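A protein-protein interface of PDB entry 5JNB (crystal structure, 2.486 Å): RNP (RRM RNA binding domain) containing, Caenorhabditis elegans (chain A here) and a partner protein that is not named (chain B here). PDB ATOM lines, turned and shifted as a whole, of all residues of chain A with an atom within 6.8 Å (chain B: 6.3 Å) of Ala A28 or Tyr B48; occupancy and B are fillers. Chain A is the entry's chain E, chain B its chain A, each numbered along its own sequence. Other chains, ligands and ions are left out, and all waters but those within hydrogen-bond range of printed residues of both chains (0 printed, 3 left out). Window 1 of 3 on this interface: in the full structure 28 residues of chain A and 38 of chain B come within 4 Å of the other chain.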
ATOM      1  N   ASP A  23      29.469 -12.637 -16.216  1.00  0.00           N
ATOM      2  CA  ASP A  23      28.037 -12.601 -16.520  1.00  0.00           C
ATOM      3  C   ASP A  23      27.497 -11.186 -16.364  1.00  0.00           C
ATOM      4  O   ASP A  23      27.533 -10.626 -15.268  1.00  0.00           O
ATOM      5  CB  ASP A  23      27.254 -13.572 -15.617  1.00  0.00           C
ATOM      6  CG  ASP A  23      25.824 -13.835 -16.112  1.00  0.00           C
ATOM      7  OD1 ASP A  23      25.303 -13.084 -16.976  1.00  0.00           O
ATOM      8  OD2 ASP A  23      25.203 -14.809 -15.623  1.00  0.00           O
ATOM      9  N   TYR A  24      26.986 -10.627 -17.463  1.00  0.00           N
ATOM     10  CA  TYR A  24      26.466  -9.261 -17.514  1.00  0.00           C
ATOM     11  C   TYR A  24      25.060  -9.250 -18.069  1.00  0.00           C
ATOM     12  O   TYR A  24      24.494  -8.191 -18.299  1.00  0.00           O
ATOM     13  CB  TYR A  24      27.355  -8.374 -18.388  1.00  0.00           C
ATOM     14  CG  TYR A  24      28.664  -7.974 -17.766  1.00  0.00           C
ATOM     15  CD1 TYR A  24      28.733  -6.906 -16.890  1.00  0.00           C
ATOM     16  CD2 TYR A  24      29.840  -8.641 -18.077  1.00  0.00           C
ATOM     17  CE1 TYR A  24      29.918  -6.530 -16.313  1.00  0.00           C
ATOM     18  CE2 TYR A  24      31.044  -8.260 -17.499  1.00  0.00           C
ATOM     19  CZ  TYR A  24      31.066  -7.208 -16.608  1.00  0.00           C
ATOM     20  OH  TYR A  24      32.250  -6.810 -16.025  1.00  0.00           O
ATOM     21  N   VAL A  25      24.515 -10.435 -18.308  1.00  0.00           N
ATOM     22  CA  VAL A  25      23.240 -10.591 -19.006  1.00  0.00           C
ATOM     23  C   VAL A  25      22.074  -9.895 -18.302  1.00  0.00           C
ATOM     24  O   VAL A  25      21.337  -9.112 -18.912  1.00  0.00           O
ATOM     25  CB  VAL A  25      22.881 -12.094 -19.184  1.00  0.00           C
ATOM     26  CG1 VAL A  25      21.461 -12.254 -19.713  1.00  0.00           C
ATOM     27  CG2 VAL A  25      23.892 -12.817 -20.096  1.00  0.00           C
ATOM     28  N   GLU A  26      21.911 -10.168 -17.012  1.00  0.00           N
ATOM     29  CA  GLU A  26      20.766  -9.640 -16.288  1.00  0.00           C
ATOM     30  C   GLU A  26      21.043  -8.190 -15.881  1.00  0.00           C
ATOM     31  O   GLU A  26      20.120  -7.370 -15.804  1.00  0.00           O
ATOM     32  CB  GLU A  26      20.432 -10.523 -15.070  1.00  0.00           C
ATOM     33  N   GLY A  27      22.313  -7.868 -15.640  1.00  0.00           N
ATOM     34  CA  GLY A  27      22.717  -6.475 -15.465  1.00  0.00           C
ATOM     35  C   GLY A  27      22.339  -5.524 -16.617  1.00  0.00           C
ATOM     36  O   GLY A  27      21.803  -4.441 -16.389  1.00  0.00           O
ATOM     37  N   ALA A  28      22.587  -5.922 -17.860  1.00  0.00           N
ATOM     38  CA  ALA A  28      22.232  -5.062 -18.987  1.00  0.00           C
ATOM     39  C   ALA A  28      20.709  -4.878 -19.084  1.00  0.00           C
ATOM     40  O   ALA A  28      20.220  -3.850 -19.562  1.00  0.00           O
ATOM     41  CB  ALA A  28      22.811  -5.627 -20.295  1.00  0.00           C
ATOM     42  N   LYS A  29      19.952  -5.859 -18.604  1.00  0.00           N
ATOM     43  CA  LYS A  29      18.494  -5.750 -18.665  1.00  0.00           C
ATOM     44  C   LYS A  29      17.946  -4.857 -17.524  1.00  0.00           C
ATOM     45  O   LYS A  29      16.999  -4.084 -17.715  1.00  0.00           O
ATOM     46  CB  LYS A  29      17.857  -7.146 -18.644  1.00  0.00           C
ATOM     47  N   ARG A  30      18.561  -4.928 -16.351  1.00  0.00           N
ATOM     48  CA  ARG A  30      18.124  -4.080 -15.246  1.00  0.00           C
ATOM     49  C   ARG A  30      18.449  -2.595 -15.466  1.00  0.00           C
ATOM     50  O   ARG A  30      17.767  -1.719 -14.942  1.00  0.00           O
ATOM     51  CB  ARG A  30      18.738  -4.579 -13.930  1.00  0.00           C
ATOM     52  CG  ARG A  30      18.063  -5.855 -13.440  1.00  0.00           C
ATOM     53  CD  ARG A  30      18.517  -6.292 -12.068  1.00  0.00           C
ATOM     54  NE  ARG A  30      19.848  -6.882 -12.092  1.00  0.00           N
ATOM     55  CZ  ARG A  30      20.954  -6.208 -11.799  1.00  0.00           C
ATOM     56  NH1 ARG A  30      20.863  -4.927 -11.460  1.00  0.00           N
ATOM     57  NH2 ARG A  30      22.144  -6.808 -11.835  1.00  0.00           N
ATOM     58  N   PHE A  31      19.472  -2.304 -16.269  1.00  0.00           N
ATOM     59  CA  PHE A  31      19.860  -0.915 -16.515  1.00  0.00           C
ATOM     60  C   PHE A  31      18.756  -0.114 -17.241  1.00  0.00           C
ATOM     61  O   PHE A  31      18.691   1.102 -17.104  1.00  0.00           O
ATOM     62  CB  PHE A  31      21.162  -0.880 -17.310  1.00  0.00           C
ATOM     63  CG  PHE A  31      21.927   0.404 -17.180  1.00  0.00           C
ATOM     64  CD1 PHE A  31      22.061   1.264 -18.267  1.00  0.00           C
ATOM     65  CD2 PHE A  31      22.529   0.753 -15.978  1.00  0.00           C
ATOM     66  CE1 PHE A  31      22.804   2.447 -18.152  1.00  0.00           C
ATOM     67  CE2 PHE A  31      23.252   1.929 -15.856  1.00  0.00           C
ATOM     68  CZ  PHE A  31      23.392   2.776 -16.960  1.00  0.00           C
ATOM     69  N   ASP A  32      17.882  -0.788 -17.985  1.00  0.00           N
ATOM     70  CA  ASP A  32      16.783  -0.103 -18.685  1.00  0.00           C
ATOM     71  C   ASP A  32      15.857   0.705 -17.756  1.00  0.00           C
ATOM     72  O   ASP A  32      15.173   1.628 -18.203  1.00  0.00           O
ATOM     73  CB  ASP A  32      15.898  -1.099 -19.454  1.00  0.00           C
ATOM     74  CG  ASP A  32      16.665  -1.948 -20.461  1.00  0.00           C
ATOM     75  OD1 ASP A  32      17.729  -1.520 -20.949  1.00  0.00           O
ATOM     76  OD2 ASP A  32      16.174  -3.052 -20.787  1.00  0.00           O
ATOM     77  N   ARG B  31      17.430  -3.501 -29.528  1.00  0.00           N
ATOM     78  CA  ARG B  31      18.597  -3.985 -28.796  1.00  0.00           C
ATOM     79  C   ARG B  31      18.508  -5.487 -28.507  1.00  0.00           C
ATOM     80  O   ARG B  31      19.497  -6.217 -28.691  1.00  0.00           O
ATOM     81  CB  ARG B  31      18.808  -3.231 -27.475  1.00  0.00           C
ATOM     82  CG  ARG B  31      19.983  -3.863 -26.743  1.00  0.00           C
ATOM     83  CD  ARG B  31      20.259  -3.353 -25.352  1.00  0.00           C
ATOM     84  NE  ARG B  31      19.109  -3.287 -24.436  1.00  0.00           N
ATOM     85  CZ  ARG B  31      18.225  -4.252 -24.232  1.00  0.00           C
ATOM     86  NH1 ARG B  31      18.330  -5.398 -24.892  1.00  0.00           N
ATOM     87  NH2 ARG B  31      17.226  -4.055 -23.366  1.00  0.00           N
ATOM     88  N   SER B  45      27.558 -12.261 -22.164  1.00  0.00           N
ATOM     89  CA  SER B  45      27.695 -10.807 -22.259  1.00  0.00           C
ATOM     90  C   SER B  45      26.385 -10.058 -21.967  1.00  0.00           C
ATOM     91  O   SER B  45      25.302 -10.633 -21.987  1.00  0.00           O
ATOM     92  CB  SER B  45      28.211 -10.418 -23.645  1.00  0.00           C
ATOM     93  OG  SER B  45      27.210 -10.613 -24.621  1.00  0.00           O
ATOM     94  N   GLY B  46      26.502  -8.768 -21.692  1.00  0.00           N
ATOM     95  CA  GLY B  46      25.343  -7.908 -21.604  1.00  0.00           C
ATOM     96  C   GLY B  46      25.432  -6.671 -22.490  1.00  0.00           C
ATOM     97  O   GLY B  46      26.474  -6.013 -22.566  1.00  0.00           O
ATOM     98  N   LEU B  47      24.318  -6.361 -23.145  1.00  0.00           N
ATOM     99  CA  LEU B  47      24.200  -5.234 -24.041  1.00  0.00           C
ATOM    100  C   LEU B  47      23.493  -4.056 -23.366  1.00  0.00           C
ATOM    101  O   LEU B  47      22.261  -4.022 -23.259  1.00  0.00           O
ATOM    102  CB  LEU B  47      23.458  -5.671 -25.314  1.00  0.00           C
ATOM    103  CG  LEU B  47      23.594  -4.768 -26.541  1.00  0.00           C
ATOM    104  CD1 LEU B  47      25.066  -4.407 -26.730  1.00  0.00           C
ATOM    105  CD2 LEU B  47      23.002  -5.406 -27.812  1.00  0.00           C
ATOM    106  N   TYR B  48      24.282  -3.091 -22.897  1.00  0.00           N
ATOM    107  CA  TYR B  48      23.743  -1.931 -22.200  1.00  0.00           C
ATOM    108  C   TYR B  48      23.364  -0.801 -23.145  1.00  0.00           C
ATOM    109  O   TYR B  48      24.052  -0.557 -24.132  1.00  0.00           O
ATOM    110  CB  TYR B  48      24.748  -1.398 -21.207  1.00  0.00           C
ATOM    111  CG  TYR B  48      24.918  -2.199 -19.925  1.00  0.00           C
ATOM    112  CD1 TYR B  48      25.563  -3.430 -19.930  1.00  0.00           C
ATOM    113  CD2 TYR B  48      24.495  -1.677 -18.705  1.00  0.00           C
ATOM    114  CE1 TYR B  48      25.763  -4.119 -18.786  1.00  0.00           C
ATOM    115  CE2 TYR B  48      24.677  -2.357 -17.550  1.00  0.00           C
ATOM    116  CZ  TYR B  48      25.314  -3.588 -17.587  1.00  0.00           C
ATOM    117  OH  TYR B  48      25.485  -4.295 -16.420  1.00  0.00           O
ATOM    118  N   VAL B  49      22.275  -0.101 -22.840  1.00  0.00           N
ATOM    119  CA  VAL B  49      21.987   1.122 -23.550  1.00  0.00           C
ATOM    120  C   VAL B  49      22.642   2.276 -22.801  1.00  0.00           C
ATOM    121  O   VAL B  49      22.389   2.465 -21.603  1.00  0.00           O
ATOM    122  CB  VAL B  49      20.496   1.386 -23.690  1.00  0.00           C
ATOM    123  CG1 VAL B  49      20.282   2.641 -24.553  1.00  0.00           C
ATOM    124  CG2 VAL B  49      19.787   0.157 -24.286  1.00  0.00           C
ATOM    125  N   VAL B  50      23.490   3.044 -23.496  1.00  0.00           N
ATOM    126  CA  VAL B  50      24.190   4.128 -22.831  1.00  0.00           C
ATOM    127  C   VAL B  50      23.965   5.427 -23.557  1.00  0.00           C
ATOM    128  O   VAL B  50      23.475   5.427 -24.677  1.00  0.00           O
ATOM    129  CB  VAL B  50      25.690   3.824 -22.701  1.00  0.00           C
ATOM    130  CG1 VAL B  50      25.882   2.599 -21.791  1.00  0.00           C
ATOM    131  CG2 VAL B  50      26.340   3.602 -24.073  1.00  0.00           C
ATOM    132  N   ASP B  65      23.200   4.373 -28.603  1.00  0.00           N
ATOM    133  CA  ASP B  65      24.545   3.965 -28.244  1.00  0.00           C
ATOM    134  C   ASP B  65      24.447   2.722 -27.341  1.00  0.00           C
ATOM    135  O   ASP B  65      23.624   2.640 -26.431  1.00  0.00           O
ATOM    136  CB  ASP B  65      25.303   5.119 -27.578  1.00  0.00           C
ATOM    137  CG  ASP B  65      25.364   6.384 -28.468  1.00  0.00           C
ATOM    138  OD1 ASP B  65      26.301   6.504 -29.293  1.00  0.00           O
ATOM    139  OD2 ASP B  65      24.485   7.273 -28.339  1.00  0.00           O
ATOM    140  N   LEU B  66      25.259   1.724 -27.633  1.00  0.00           N
ATOM    141  CA  LEU B  66      25.172   0.471 -26.933  1.00  0.00           C
ATOM    142  C   LEU B  66      26.542   0.104 -26.431  1.00  0.00           C
ATOM    143  O   LEU B  66      27.543   0.367 -27.086  1.00  0.00           O
ATOM    144  CB  LEU B  66      24.630  -0.642 -27.836  1.00  0.00           C
ATOM    145  CG  LEU B  66      23.204  -0.553 -28.377  1.00  0.00           C
ATOM    146  CD1 LEU B  66      22.932  -1.758 -29.230  1.00  0.00           C
ATOM    147  CD2 LEU B  66      22.199  -0.440 -27.253  1.00  0.00           C
ATOM    148  N   CYS B  67      26.585  -0.521 -25.266  1.00  0.00           N
ATOM    149  CA  CYS B  67      27.847  -0.913 -24.690  1.00  0.00           C
ATOM    150  C   CYS B  67      27.808  -2.406 -24.402  1.00  0.00           C
ATOM    151  O   CYS B  67      27.043  -2.877 -23.560  1.00  0.00           O
ATOM    152  CB  CYS B  67      28.145  -0.098 -23.426  1.00  0.00           C
ATOM    153  SG  CYS B  67      29.706  -0.542 -22.673  1.00  0.00           S
ATOM    154  N   LEU B  68      28.617  -3.152 -25.143  1.00  0.00           N
ATOM    155  CA  LEU B  68      28.664  -4.586 -24.981  1.00  0.00           C
ATOM    156  C   LEU B  68      29.662  -4.925 -23.901  1.00  0.00           C
ATOM    157  O   LEU B  68      30.867  -4.784 -24.109  1.00  0.00           O
ATOM    158  CB  LEU B  68      29.048  -5.279 -26.283  1.00  0.00           C
ATOM    159  CG  LEU B  68      29.011  -6.798 -26.154  1.00  0.00           C
ATOM    160  CD1 LEU B  68      27.612  -7.266 -25.695  1.00  0.00           C
ATOM    161  CD2 LEU B  68      29.397  -7.459 -27.459  1.00  0.00           C
ATOM    162  N   MET B  69      29.164  -5.363 -22.749  1.00  0.00           N
ATOM    163  CA  MET B  69      30.044  -5.783 -21.680  1.00  0.00           C
ATOM    164  C   MET B  69      30.278  -7.298 -21.736  1.00  0.00           C
ATOM    165  O   MET B  69      29.335  -8.077 -21.857  1.00  0.00           O
ATOM    166  CB  MET B  69      29.471  -5.346 -20.316  1.00  0.00           C
ATOM    167  CG  MET B  69      30.548  -4.902 -19.323  1.00  0.00           C
ATOM    168  SD  MET B  69      31.361  -3.381 -19.852  1.00  0.00           S
ATOM    169  CE  MET B  69      29.936  -2.659 -20.506  1.00  0.00           C
ATOM    170  N   LEU B 126      27.888   1.070 -31.309  1.00  0.00           N
ATOM    171  CA  LEU B 126      28.240   0.013 -30.375  1.00  0.00           C
ATOM    172  C   LEU B 126      29.719   0.067 -30.019  1.00  0.00           C
ATOM    173  O   LEU B 126      30.588   0.044 -30.901  1.00  0.00           O
ATOM    174  CB  LEU B 126      27.915  -1.372 -30.960  1.00  0.00           C
ATOM    175  CG  LEU B 126      28.336  -2.536 -30.034  1.00  0.00           C
ATOM    176  CD1 LEU B 126      27.350  -2.668 -28.867  1.00  0.00           C
ATOM    177  CD2 LEU B 126      28.488  -3.867 -30.754  1.00  0.00           C
ATOM    178  N   ILE B 134      28.683   3.369 -18.916  1.00  0.00           N
ATOM    179  CA  ILE B 134      27.564   2.969 -18.060  1.00  0.00           C
ATOM    180  C   ILE B 134      27.523   3.842 -16.801  1.00  0.00           C
ATOM    181  O   ILE B 134      26.486   4.405 -16.496  1.00  0.00           O
ATOM    182  CB  ILE B 134      27.650   1.502 -17.670  1.00  0.00           C
ATOM    183  CG1 ILE B 134      27.437   0.614 -18.888  1.00  0.00           C
ATOM    184  CG2 ILE B 134      26.611   1.172 -16.624  1.00  0.00           C
ATOM    185  CD1 ILE B 134      27.922  -0.777 -18.641  1.00  0.00           C
ATOM    186  N   VAL B 212      29.437  -2.186 -11.918  1.00  0.00           N
ATOM    187  CA  VAL B 212      28.285  -1.609 -12.614  1.00  0.00           C
ATOM    188  C   VAL B 212      27.089  -2.556 -12.624  1.00  0.00           C
ATOM    189  O   VAL B 212      25.973  -2.169 -13.003  1.00  0.00           O
ATOM    190  CB  VAL B 212      28.597  -1.233 -14.094  1.00  0.00           C
ATOM    191  CG1 VAL B 212      29.789  -0.333 -14.172  1.00  0.00           C
ATOM    192  CG2 VAL B 212      28.756  -2.500 -14.961  1.00  0.00           C
ATOM    193  N   ARG B 213      27.326  -3.810 -12.256  1.00  0.00           N
ATOM    194  CA  ARG B 213      26.230  -4.760 -12.156  1.00  0.00           C
ATOM    195  C   ARG B 213      25.417  -4.558 -10.860  1.00  0.00           C
ATOM    196  O   ARG B 213      24.341  -5.134 -10.703  1.00  0.00           O
ATOM    197  CB  ARG B 213      26.763  -6.190 -12.235  1.00  0.00           C
ATOM    198  CG  ARG B 213      27.150  -6.622 -13.638  1.00  0.00           C
ATOM    199  CD  ARG B 213      27.839  -7.963 -13.580  1.00  0.00           C
ATOM    200  NE  ARG B 213      29.205  -7.865 -13.065  1.00  0.00           N
ATOM    201  CZ  ARG B 213      30.042  -8.897 -13.012  1.00  0.00           C
ATOM    202  NH1 ARG B 213      29.628 -10.079 -13.423  1.00  0.00           N
ATOM    203  NH2 ARG B 213      31.272  -8.762 -12.540  1.00  0.00           N
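Of the 16 printed residues of chain B, 9 touch a printed residue of chain A.
Hydrophobic or aromatic side chains of chain B within 4 Å of the printed part of chain A: Tyr B48, Met B69 and Ile B134.
Printed residues of chain A that touch a printed residue of chain B: Asp A23, Tyr A24, Val A25, Gly A27, Ala A28, Arg A30, Phe A31 and Asp A32.
Hydrophobic or aromatic side chains of chain A within 4 Å of the printed part of chain B: Tyr A24, Val A25, Ala A28 and Phe A31.
Among the printed residues, 14 pairs touch across the chains.
Among the printed residues, Asp or Glu carboxylates within 4 Å of a Lys or Arg side-chain nitrogen of the other chain: Asp A32 with Arg B31.
Among the printed residues, pairs that only touch across the chains: Tyr A24 with Gly B46 (3.4 Å), Tyr A24 with Met B69 (3.5 Å), Tyr A24 with Arg B213 (3.6 Å), Val A25 with Ser B45 (3.2 Å), Gly A27 with Tyr B48 (3.4 Å), Ala A28 with Gly B46 (3.6 Å), Ala A28 with Leu B47 (3.3 Å), Ala A28 with Tyr B48 (3.5 Å), Phe A31 with Tyr B48 (3.6 Å), Phe A31 with Val B49 (3.5 Å) and Phe A31 with Ile B134 (3.5 Å).
The side-chain carboxylate of Asp A32 lies within salt-bridge range of the guanidinium group of Arg B31 (3.0 Å).
The backbone carbonyl oxygen (O) of Arg B213 sits at hydrogen-bond distance from the guanidinium group (NH2) of Arg A30.
NH1 of Arg B213 lies within hydrogen-bond range of O of Asp A23 (2.8 Å).
Of the printed residues of chain B, Asp A23 touches Arg B213.
Ala A28 touches three residues of chain B.
Lys A29 touches none of the printed residues of chain B.
Of the printed residues of chain A, Leu B47 touches Ala A28.
Of chain A, only Gly A27, Ala A28 and Phe A31 come within 4 Å of Tyr B48.
Printed residues of chain A within 4 Å of Val B49: Phe A31.
The nearest residue of chain A that does not touch Tyr B48 is Tyr A24 (4.2 Å).
The nearest printed residue of chain A that does not touch Arg B213 is Gly A27 (4.8 Å).
O of Leu B47 sits close to NE of Arg B31, 3.4 Å away.
O of Tyr B48 sits at hydrogen-bond distance from N of Cys B67, at 2.8 Å.
OD1 of Asp A23 is in hydrogen-bond range of N of Val A25.
The backbone carbonyl oxygen (O) of Gly B46 sits at hydrogen-bond distance from the backbone NH (N) of Met B69 (2.8 Å).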
